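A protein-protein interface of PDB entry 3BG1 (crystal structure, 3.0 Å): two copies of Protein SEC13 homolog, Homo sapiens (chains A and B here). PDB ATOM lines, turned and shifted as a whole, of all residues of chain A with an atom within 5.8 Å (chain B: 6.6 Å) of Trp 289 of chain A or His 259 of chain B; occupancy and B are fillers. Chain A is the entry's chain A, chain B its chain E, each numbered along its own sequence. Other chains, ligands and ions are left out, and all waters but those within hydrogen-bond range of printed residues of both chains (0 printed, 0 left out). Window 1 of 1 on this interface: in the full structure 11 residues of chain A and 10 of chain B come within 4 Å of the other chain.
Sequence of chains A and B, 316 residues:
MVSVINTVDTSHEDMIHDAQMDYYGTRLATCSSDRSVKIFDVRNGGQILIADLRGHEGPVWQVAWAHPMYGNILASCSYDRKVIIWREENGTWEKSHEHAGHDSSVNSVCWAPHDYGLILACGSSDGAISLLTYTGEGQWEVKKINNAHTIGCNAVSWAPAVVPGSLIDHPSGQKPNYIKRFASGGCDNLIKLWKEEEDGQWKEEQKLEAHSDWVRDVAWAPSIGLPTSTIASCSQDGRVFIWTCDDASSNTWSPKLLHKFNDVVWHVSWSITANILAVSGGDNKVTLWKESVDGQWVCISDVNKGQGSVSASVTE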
ATOM      1  N   LEU A 258      18.792 -32.989  25.604  1.00  0.00           N
ATOM      2  CA  LEU A 258      18.964 -32.269  24.356  1.00  0.00           C
ATOM      3  C   LEU A 258      18.414 -30.873  24.539  1.00  0.00           C
ATOM      4  O   LEU A 258      19.122 -29.890  24.352  1.00  0.00           O
ATOM      5  CB  LEU A 258      18.227 -32.985  23.221  1.00  0.00           C
ATOM      6  CG  LEU A 258      18.275 -32.376  21.814  1.00  0.00           C
ATOM      7  CD1 LEU A 258      19.611 -31.733  21.562  1.00  0.00           C
ATOM      8  CD2 LEU A 258      17.999 -33.469  20.782  1.00  0.00           C
ATOM      9  N   HIS A 259      17.146 -30.789  24.925  1.00  0.00           N
ATOM     10  CA  HIS A 259      16.517 -29.493  25.140  1.00  0.00           C
ATOM     11  C   HIS A 259      15.107 -29.687  25.673  1.00  0.00           C
ATOM     12  O   HIS A 259      14.552 -30.788  25.618  1.00  0.00           O
ATOM     13  CB  HIS A 259      16.488 -28.719  23.815  1.00  0.00           C
ATOM     14  CG  HIS A 259      16.209 -27.259  23.963  1.00  0.00           C
ATOM     15  ND1 HIS A 259      15.050 -26.673  23.506  1.00  0.00           N
ATOM     16  CD2 HIS A 259      16.952 -26.260  24.498  1.00  0.00           C
ATOM     17  CE1 HIS A 259      15.089 -25.375  23.750  1.00  0.00           C
ATOM     18  NE2 HIS A 259      16.233 -25.100  24.351  1.00  0.00           N
ATOM     19  N   PHE A 261      11.238 -27.763  25.624  1.00  0.00           N
ATOM     20  CA  PHE A 261      10.392 -26.713  25.083  1.00  0.00           C
ATOM     21  C   PHE A 261       9.211 -26.662  26.020  1.00  0.00           C
ATOM     22  O   PHE A 261       8.906 -27.663  26.659  1.00  0.00           O
ATOM     23  CB  PHE A 261       9.933 -27.093  23.687  1.00  0.00           C
ATOM     24  CG  PHE A 261      10.961 -27.843  22.913  1.00  0.00           C
ATOM     25  CD1 PHE A 261      11.100 -29.213  23.074  1.00  0.00           C
ATOM     26  CD2 PHE A 261      11.827 -27.174  22.062  1.00  0.00           C
ATOM     27  CE1 PHE A 261      12.090 -29.907  22.398  1.00  0.00           C
ATOM     28  CE2 PHE A 261      12.819 -27.857  21.382  1.00  0.00           C
ATOM     29  CZ  PHE A 261      12.954 -29.226  21.551  1.00  0.00           C
ATOM     30  N   ASN A 275      23.862 -38.271  12.016  1.00  0.00           N
ATOM     31  CA  ASN A 275      23.183 -38.603  13.235  1.00  0.00           C
ATOM     32  C   ASN A 275      22.516 -37.307  13.686  1.00  0.00           C
ATOM     33  O   ASN A 275      22.517 -36.943  14.857  1.00  0.00           O
ATOM     34  CB  ASN A 275      24.175 -39.212  14.243  1.00  0.00           C
ATOM     35  CG  ASN A 275      24.834 -40.477  13.691  1.00  0.00           C
ATOM     36  OD1 ASN A 275      24.169 -41.292  13.047  1.00  0.00           O
ATOM     37  ND2 ASN A 275      26.133 -40.643  13.931  1.00  0.00           N
ATOM     38  N   ILE A 276      21.936 -36.605  12.712  1.00  0.00           N
ATOM     39  CA  ILE A 276      21.212 -35.373  13.007  1.00  0.00           C
ATOM     40  C   ILE A 276      19.804 -35.676  13.469  1.00  0.00           C
ATOM     41  O   ILE A 276      19.078 -36.488  12.888  1.00  0.00           O
ATOM     42  CB  ILE A 276      21.150 -34.465  11.814  1.00  0.00           C
ATOM     43  CG1 ILE A 276      22.581 -34.148  11.418  1.00  0.00           C
ATOM     44  CG2 ILE A 276      20.354 -33.206  12.160  1.00  0.00           C
ATOM     45  CD1 ILE A 276      22.693 -33.218  10.304  1.00  0.00           C
ATOM     46  N   LEU A 277      19.406 -35.021  14.534  1.00  0.00           N
ATOM     47  CA  LEU A 277      18.099 -35.319  15.031  1.00  0.00           C
ATOM     48  C   LEU A 277      17.086 -34.324  14.544  1.00  0.00           C
ATOM     49  O   LEU A 277      17.274 -33.106  14.672  1.00  0.00           O
ATOM     50  CB  LEU A 277      18.102 -35.327  16.551  1.00  0.00           C
ATOM     51  CG  LEU A 277      16.874 -35.984  17.171  1.00  0.00           C
ATOM     52  CD1 LEU A 277      16.903 -37.457  16.815  1.00  0.00           C
ATOM     53  CD2 LEU A 277      16.866 -35.776  18.682  1.00  0.00           C
ATOM     54  N   ALA A 278      16.008 -34.852  13.975  1.00  0.00           N
ATOM     55  CA  ALA A 278      14.938 -34.006  13.511  1.00  0.00           C
ATOM     56  C   ALA A 278      13.962 -33.995  14.668  1.00  0.00           C
ATOM     57  O   ALA A 278      13.356 -35.028  14.975  1.00  0.00           O
ATOM     58  CB  ALA A 278      14.295 -34.610  12.304  1.00  0.00           C
ATOM     59  N   VAL A 279      13.813 -32.850  15.316  1.00  0.00           N
ATOM     60  CA  VAL A 279      12.904 -32.779  16.446  1.00  0.00           C
ATOM     61  C   VAL A 279      11.569 -32.158  16.094  1.00  0.00           C
ATOM     62  O   VAL A 279      11.452 -30.935  15.945  1.00  0.00           O
ATOM     63  CB  VAL A 279      13.508 -31.983  17.614  1.00  0.00           C
ATOM     64  CG1 VAL A 279      12.537 -31.966  18.784  1.00  0.00           C
ATOM     65  CG2 VAL A 279      14.811 -32.612  18.039  1.00  0.00           C
ATOM     66  N   THR A 287      12.776 -28.911  14.344  1.00  0.00           N
ATOM     67  CA  THR A 287      14.170 -28.509  14.507  1.00  0.00           C
ATOM     68  C   THR A 287      15.193 -29.573  14.167  1.00  0.00           C
ATOM     69  O   THR A 287      14.920 -30.771  14.210  1.00  0.00           O
ATOM     70  CB  THR A 287      14.394 -28.063  15.950  1.00  0.00           C
ATOM     71  OG1 THR A 287      13.367 -28.628  16.789  1.00  0.00           O
ATOM     72  CG2 THR A 287      14.337 -26.568  16.046  1.00  0.00           C
ATOM     73  N   LEU A 288      16.386 -29.135  13.834  1.00  0.00           N
ATOM     74  CA  LEU A 288      17.416 -30.090  13.529  1.00  0.00           C
ATOM     75  C   LEU A 288      18.522 -29.946  14.546  1.00  0.00           C
ATOM     76  O   LEU A 288      18.811 -28.833  14.992  1.00  0.00           O
ATOM     77  CB  LEU A 288      17.948 -29.860  12.120  1.00  0.00           C
ATOM     78  CG  LEU A 288      16.990 -30.316  11.020  1.00  0.00           C
ATOM     79  CD1 LEU A 288      17.788 -30.649   9.770  1.00  0.00           C
ATOM     80  CD2 LEU A 288      16.223 -31.570  11.460  1.00  0.00           C
ATOM     81  N   TRP A 289      19.122 -31.062  14.948  1.00  0.00           N
ATOM     82  CA  TRP A 289      20.207 -30.982  15.903  1.00  0.00           C
ATOM     83  C   TRP A 289      21.337 -31.882  15.549  1.00  0.00           C
ATOM     84  O   TRP A 289      21.153 -32.982  15.006  1.00  0.00           O
ATOM     85  CB  TRP A 289      19.740 -31.340  17.283  1.00  0.00           C
ATOM     86  CG  TRP A 289      18.558 -30.605  17.680  1.00  0.00           C
ATOM     87  CD1 TRP A 289      17.291 -30.805  17.242  1.00  0.00           C
ATOM     88  CD2 TRP A 289      18.492 -29.579  18.660  1.00  0.00           C
ATOM     89  NE1 TRP A 289      16.422 -29.969  17.907  1.00  0.00           N
ATOM     90  CE2 TRP A 289      17.140 -29.207  18.784  1.00  0.00           C
ATOM     91  CE3 TRP A 289      19.447 -28.942  19.453  1.00  0.00           C
ATOM     92  CZ2 TRP A 289      16.715 -28.230  19.664  1.00  0.00           C
ATOM     93  CZ3 TRP A 289      19.031 -27.964  20.334  1.00  0.00           C
ATOM     94  CH2 TRP A 289      17.675 -27.618  20.438  1.00  0.00           C
ATOM     95  N   LYS A 290      22.502 -31.347  15.823  1.00  0.00           N
ATOM     96  CA  LYS A 290      23.732 -32.062  15.631  1.00  0.00           C
ATOM     97  C   LYS A 290      24.553 -31.855  16.899  1.00  0.00           C
ATOM     98  O   LYS A 290      24.633 -30.748  17.433  1.00  0.00           O
ATOM     99  CB  LYS A 290      24.487 -31.537  14.417  1.00  0.00           C
ATOM    100  CG  LYS A 290      25.627 -32.440  14.039  1.00  0.00           C
ATOM    101  CD  LYS A 290      26.196 -32.123  12.692  1.00  0.00           C
ATOM    102  CE  LYS A 290      27.113 -33.247  12.289  1.00  0.00           C
ATOM    103  NZ  LYS A 290      27.689 -33.018  10.954  1.00  0.00           N
ATOM    104  N   GLU A 291      25.136 -32.941  17.390  1.00  0.00           N
ATOM    105  CA  GLU A 291      25.952 -32.910  18.590  1.00  0.00           C
ATOM    106  C   GLU A 291      27.289 -32.289  18.223  1.00  0.00           C
ATOM    107  O   GLU A 291      27.977 -32.796  17.340  1.00  0.00           O
ATOM    108  CB  GLU A 291      26.140 -34.342  19.098  1.00  0.00           C
ATOM    109  CG  GLU A 291      27.100 -34.503  20.257  1.00  0.00           C
ATOM    110  CD  GLU A 291      26.948 -35.850  20.921  1.00  0.00           C
ATOM    111  OE1 GLU A 291      26.882 -36.863  20.190  1.00  0.00           O
ATOM    112  OE2 GLU A 291      26.890 -35.891  22.169  1.00  0.00           O
ATOM    113  N   TRP A 297      24.416 -30.611  22.491  1.00  0.00           N
ATOM    114  CA  TRP A 297      23.699 -30.666  21.215  1.00  0.00           C
ATOM    115  C   TRP A 297      23.189 -29.275  20.867  1.00  0.00           C
ATOM    116  O   TRP A 297      22.750 -28.519  21.751  1.00  0.00           O
ATOM    117  CB  TRP A 297      22.481 -31.591  21.250  1.00  0.00           C
ATOM    118  CG  TRP A 297      22.727 -33.056  21.246  1.00  0.00           C
ATOM    119  CD1 TRP A 297      22.845 -33.858  22.337  1.00  0.00           C
ATOM    120  CD2 TRP A 297      22.860 -33.915  20.102  1.00  0.00           C
ATOM    121  NE1 TRP A 297      23.041 -35.165  21.955  1.00  0.00           N
ATOM    122  CE2 TRP A 297      23.057 -35.229  20.585  1.00  0.00           C
ATOM    123  CE3 TRP A 297      22.833 -33.708  18.722  1.00  0.00           C
ATOM    124  CZ2 TRP A 297      23.232 -36.332  19.731  1.00  0.00           C
ATOM    125  CZ3 TRP A 297      23.009 -34.808  17.873  1.00  0.00           C
ATOM    126  CH2 TRP A 297      23.205 -36.098  18.387  1.00  0.00           C
ATOM    127  N   VAL A 298      23.235 -28.957  19.572  1.00  0.00           N
ATOM    128  CA  VAL A 298      22.766 -27.676  19.071  1.00  0.00           C
ATOM    129  C   VAL A 298      21.753 -27.787  17.973  1.00  0.00           C
ATOM    130  O   VAL A 298      21.635 -28.812  17.289  1.00  0.00           O
ATOM    131  CB  VAL A 298      23.870 -26.831  18.494  1.00  0.00           C
ATOM    132  CG1 VAL A 298      24.462 -25.974  19.575  1.00  0.00           C
ATOM    133  CG2 VAL A 298      24.898 -27.711  17.850  1.00  0.00           C
ATOM    134  N   CYS A 299      21.034 -26.688  17.820  1.00  0.00           N
ATOM    135  CA  CYS A 299      20.009 -26.557  16.817  1.00  0.00           C
ATOM    136  C   CYS A 299      20.686 -26.014  15.568  1.00  0.00           C
ATOM    137  O   CYS A 299      21.212 -24.910  15.601  1.00  0.00           O
ATOM    138  CB  CYS A 299      18.967 -25.567  17.315  1.00  0.00           C
ATOM    139  SG  CYS A 299      17.535 -25.474  16.273  1.00  0.00           S
ATOM    140  N   ILE A 300      20.696 -26.768  14.473  1.00  0.00           N
ATOM    141  CA  ILE A 300      21.339 -26.263  13.262  1.00  0.00           C
ATOM    142  C   ILE A 300      20.465 -25.325  12.471  1.00  0.00           C
ATOM    143  O   ILE A 300      20.965 -24.462  11.747  1.00  0.00           O
ATOM    144  CB  ILE A 300      21.745 -27.353  12.274  1.00  0.00           C
ATOM    145  CG1 ILE A 300      20.930 -28.611  12.530  1.00  0.00           C
ATOM    146  CG2 ILE A 300      23.245 -27.554  12.298  1.00  0.00           C
ATOM    147  CD1 ILE A 300      21.541 -29.899  11.890  1.00  0.00           C
ATOM    148  N   GLY B 238      28.730 -18.604  21.619  1.00  0.00           N
ATOM    149  CA  GLY B 238      27.328 -18.873  21.388  1.00  0.00           C
ATOM    150  C   GLY B 238      26.609 -19.545  22.541  1.00  0.00           C
ATOM    151  O   GLY B 238      25.719 -20.377  22.340  1.00  0.00           O
ATOM    152  N   ARG B 239      26.996 -19.186  23.758  1.00  0.00           N
ATOM    153  CA  ARG B 239      26.368 -19.745  24.947  1.00  0.00           C
ATOM    154  C   ARG B 239      25.825 -18.568  25.744  1.00  0.00           C
ATOM    155  O   ARG B 239      26.351 -17.452  25.668  1.00  0.00           O
ATOM    156  CB  ARG B 239      27.394 -20.487  25.831  1.00  0.00           C
ATOM    157  CG  ARG B 239      28.294 -21.532  25.169  1.00  0.00           C
ATOM    158  CD  ARG B 239      29.359 -21.990  26.163  1.00  0.00           C
ATOM    159  NE  ARG B 239      30.581 -22.414  25.493  1.00  0.00           N
ATOM    160  CZ  ARG B 239      30.751 -23.601  24.919  1.00  0.00           C
ATOM    161  NH1 ARG B 239      29.769 -24.498  24.939  1.00  0.00           N
ATOM    162  NH2 ARG B 239      31.904 -23.885  24.315  1.00  0.00           N
ATOM    163  N   VAL B 240      24.779 -18.810  26.516  1.00  0.00           N
ATOM    164  CA  VAL B 240      24.232 -17.750  27.340  1.00  0.00           C
ATOM    165  C   VAL B 240      24.183 -18.288  28.757  1.00  0.00           C
ATOM    166  O   VAL B 240      23.543 -19.313  29.017  1.00  0.00           O
ATOM    167  CB  VAL B 240      22.827 -17.361  26.889  1.00  0.00           C
ATOM    168  CG1 VAL B 240      22.371 -16.119  27.635  1.00  0.00           C
ATOM    169  CG2 VAL B 240      22.822 -17.120  25.397  1.00  0.00           C
ATOM    170  N   PHE B 241      24.880 -17.611  29.666  1.00  0.00           N
ATOM    171  CA  PHE B 241      24.915 -18.042  31.055  1.00  0.00           C
ATOM    172  C   PHE B 241      24.179 -17.122  31.984  1.00  0.00           C
ATOM    173  O   PHE B 241      24.109 -15.902  31.779  1.00  0.00           O
ATOM    174  CB  PHE B 241      26.358 -18.170  31.558  1.00  0.00           C
ATOM    175  CG  PHE B 241      27.120 -19.305  30.937  1.00  0.00           C
ATOM    176  CD1 PHE B 241      28.384 -19.092  30.393  1.00  0.00           C
ATOM    177  CD2 PHE B 241      26.568 -20.582  30.872  1.00  0.00           C
ATOM    178  CE1 PHE B 241      29.088 -20.128  29.785  1.00  0.00           C
ATOM    179  CE2 PHE B 241      27.263 -21.628  30.267  1.00  0.00           C
ATOM    180  CZ  PHE B 241      28.526 -21.399  29.721  1.00  0.00           C
ATOM    181  N   ILE B 242      23.705 -17.743  33.047  1.00  0.00           N
ATOM    182  CA  ILE B 242      22.999 -17.039  34.076  1.00  0.00           C
ATOM    183  C   ILE B 242      23.704 -17.386  35.373  1.00  0.00           C
ATOM    184  O   ILE B 242      23.601 -18.491  35.909  1.00  0.00           O
ATOM    185  CB  ILE B 242      21.559 -17.452  34.055  1.00  0.00           C
ATOM    186  CG1 ILE B 242      21.041 -17.193  32.666  1.00  0.00           C
ATOM    187  CG2 ILE B 242      20.742 -16.629  34.997  1.00  0.00           C
ATOM    188  CD1 ILE B 242      20.075 -18.195  32.259  1.00  0.00           C
ATOM    189  N   LYS B 256      25.132 -21.078  35.051  1.00  0.00           N
ATOM    190  CA  LYS B 256      24.228 -22.127  34.597  1.00  0.00           C
ATOM    191  C   LYS B 256      23.980 -21.833  33.124  1.00  0.00           C
ATOM    192  O   LYS B 256      23.750 -20.678  32.759  1.00  0.00           O
ATOM    193  CB  LYS B 256      22.920 -22.062  35.380  1.00  0.00           C
ATOM    194  CG  LYS B 256      21.981 -23.224  35.127  1.00  0.00           C
ATOM    195  CD  LYS B 256      20.794 -23.132  36.061  1.00  0.00           C
ATOM    196  CE  LYS B 256      19.958 -24.385  36.018  1.00  0.00           C
ATOM    197  NZ  LYS B 256      18.967 -24.346  37.118  1.00  0.00           N
ATOM    198  N   LEU B 257      24.029 -22.859  32.279  1.00  0.00           N
ATOM    199  CA  LEU B 257      23.832 -22.655  30.839  1.00  0.00           C
ATOM    200  C   LEU B 257      22.397 -22.513  30.358  1.00  0.00           C
ATOM    201  O   LEU B 257      21.563 -23.397  30.561  1.00  0.00           O
ATOM    202  CB  LEU B 257      24.491 -23.773  30.027  1.00  0.00           C
ATOM    203  CG  LEU B 257      24.244 -23.653  28.522  1.00  0.00           C
ATOM    204  CD1 LEU B 257      24.654 -22.270  28.034  1.00  0.00           C
ATOM    205  CD2 LEU B 257      25.023 -24.726  27.791  1.00  0.00           C
ATOM    206  N   LEU B 258      22.128 -21.397  29.691  1.00  0.00           N
ATOM    207  CA  LEU B 258      20.803 -21.133  29.161  1.00  0.00           C
ATOM    208  C   LEU B 258      20.642 -21.926  27.885  1.00  0.00           C
ATOM    209  O   LEU B 258      19.727 -22.735  27.762  1.00  0.00           O
ATOM    210  CB  LEU B 258      20.626 -19.640  28.880  1.00  0.00           C
ATOM    211  CG  LEU B 258      19.292 -19.153  28.303  1.00  0.00           C
ATOM    212  CD1 LEU B 258      18.150 -19.959  28.863  1.00  0.00           C
ATOM    213  CD2 LEU B 258      19.111 -17.668  28.628  1.00  0.00           C
ATOM    214  N   HIS B 259      21.546 -21.705  26.940  1.00  0.00           N
ATOM    215  CA  HIS B 259      21.490 -22.425  25.674  1.00  0.00           C
ATOM    216  C   HIS B 259      22.693 -22.057  24.819  1.00  0.00           C
ATOM    217  O   HIS B 259      23.396 -21.076  25.094  1.00  0.00           O
ATOM    218  CB  HIS B 259      20.189 -22.065  24.946  1.00  0.00           C
ATOM    219  CG  HIS B 259      19.835 -22.989  23.827  1.00  0.00           C
ATOM    220  ND1 HIS B 259      19.840 -22.596  22.508  1.00  0.00           N
ATOM    221  CD2 HIS B 259      19.441 -24.285  23.833  1.00  0.00           C
ATOM    222  CE1 HIS B 259      19.464 -23.609  21.748  1.00  0.00           C
ATOM    223  NE2 HIS B 259      19.217 -24.646  22.529  1.00  0.00           N
ATOM    224  N   LYS B 260      22.948 -22.858  23.798  1.00  0.00           N
ATOM    225  CA  LYS B 260      24.050 -22.573  22.903  1.00  0.00           C
ATOM    226  C   LYS B 260      23.539 -22.684  21.479  1.00  0.00           C
ATOM    227  O   LYS B 260      22.875 -23.660  21.124  1.00  0.00           O
ATOM    228  CB  LYS B 260      25.211 -23.554  23.097  1.00  0.00           C
ATOM    229  CG  LYS B 260      26.448 -23.157  22.295  1.00  0.00           C
ATOM    230  CD  LYS B 260      27.421 -24.302  22.077  1.00  0.00           C
ATOM    231  CE  LYS B 260      28.608 -23.844  21.213  1.00  0.00           C
ATOM    232  NZ  LYS B 260      29.537 -24.953  20.819  1.00  0.00           N
ATOM    233  N   PHE B 261      23.840 -21.673  20.671  1.00  0.00           N
ATOM    234  CA  PHE B 261      23.431 -21.657  19.279  1.00  0.00           C
ATOM    235  C   PHE B 261      24.717 -21.802  18.506  1.00  0.00           C
ATOM    236  O   PHE B 261      25.768 -21.440  19.016  1.00  0.00           O
ATOM    237  CB  PHE B 261      22.778 -20.325  18.951  1.00  0.00           C
ATOM    238  CG  PHE B 261      21.982 -19.768  20.082  1.00  0.00           C
ATOM    239  CD1 PHE B 261      22.601 -19.041  21.087  1.00  0.00           C
ATOM    240  CD2 PHE B 261      20.617 -20.014  20.170  1.00  0.00           C
ATOM    241  CE1 PHE B 261      21.872 -18.569  22.170  1.00  0.00           C
ATOM    242  CE2 PHE B 261      19.881 -19.548  21.250  1.00  0.00           C
ATOM    243  CZ  PHE B 261      20.509 -18.824  22.251  1.00  0.00           C
ATOM    244  N   VAL B 265      25.978 -14.648  19.894  1.00  0.00           N
ATOM    245  CA  VAL B 265      24.827 -13.965  20.485  1.00  0.00           C
ATOM    246  C   VAL B 265      25.319 -12.548  20.729  1.00  0.00           C
ATOM    247  O   VAL B 265      26.359 -12.352  21.366  1.00  0.00           O
ATOM    248  CB  VAL B 265      24.385 -14.607  21.803  1.00  0.00           C
ATOM    249  CG1 VAL B 265      23.355 -13.712  22.510  1.00  0.00           C
ATOM    250  CG2 VAL B 265      23.800 -16.000  21.521  1.00  0.00           C
ATOM    251  N   TRP B 289      13.153 -15.952  27.011  1.00  0.00           N
ATOM    252  CA  TRP B 289      13.281 -17.066  27.928  1.00  0.00           C
ATOM    253  C   TRP B 289      12.815 -16.723  29.307  1.00  0.00           C
ATOM    254  O   TRP B 289      12.955 -15.576  29.763  1.00  0.00           O
ATOM    255  CB  TRP B 289      14.706 -17.522  28.023  1.00  0.00           C
ATOM    256  CG  TRP B 289      15.301 -17.763  26.729  1.00  0.00           C
ATOM    257  CD1 TRP B 289      15.709 -16.830  25.830  1.00  0.00           C
ATOM    258  CD2 TRP B 289      15.646 -19.025  26.182  1.00  0.00           C
ATOM    259  NE1 TRP B 289      16.304 -17.436  24.754  1.00  0.00           N
ATOM    260  CE2 TRP B 289      16.278 -18.788  24.944  1.00  0.00           C
ATOM    261  CE3 TRP B 289      15.488 -20.344  26.621  1.00  0.00           C
ATOM    262  CZ2 TRP B 289      16.754 -19.817  24.138  1.00  0.00           C
ATOM    263  CZ3 TRP B 289      15.958 -21.376  25.821  1.00  0.00           C
ATOM    264  CH2 TRP B 289      16.587 -21.106  24.589  1.00  0.00           C
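The backbone NH of Val 240 of chain B sits at hydrogen-bond distance from the backbone carbonyl oxygen of His 259 of chain B (3.0 Å). The backbone NH (N) of Leu 277 of chain A sits at hydrogen-bond distance from the backbone carbonyl oxygen (O) of Trp 289 of chain A (2.7 Å). The backbone NH (N) of Lys 290 of chain A sits at hydrogen-bond distance from the backbone carbonyl oxygen (O) of Val 298 of chain A, at 3.1 Å.
His 259 of chain A touches His 259 of chain B. Trp 289 of chain A touches His 259 of chain B (CH2 to NE2, 3.9 Å). CG1 of Val 298 of chain A touches O of Lys 260 of chain B, 3.2 Å away.
Printed residues of chain B within 4 Å of His 259 of chain A: His 259. Asn 275 of chain A touches none of the printed residues of chain B. Trp 289 of chain A touches just one residue of chain B: His 259 (3.9 Å). Of chain A, only His 259 and Trp 289 come within 4 Å of His 259 of chain B. Of the printed residues of chain A, Lys 260 of chain B touches Val 298 (3.2 Å). The nearest residue of chain B that does not touch Trp 289 of chain A is Lys 260 of chain B (5.8 Å). The nearest printed residue of chain B that does not touch Val 298 of chain A is Phe 261 of chain B (4.3 Å).
Among the printed residues, 3 pairs touch across the chains. Among the printed residues, no Asp or Glu carboxylate lies within 4 Å of a Lys or Arg side-chain nitrogen of the other chain.
His 259 of chain B touches its own counterpart, His 259 of chain A. Trp 289 of chain A touches His 259 of chain B, but with the chains exchanged His 259 of chain A does not touch Trp 289 of chain B (4.01 Å). Positions printed for both chains: 258, 259, 261 and 289. Of the 3 pairs that touch across the chains among the printed residues, 1 has its exchanged pair printed and touching as well.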
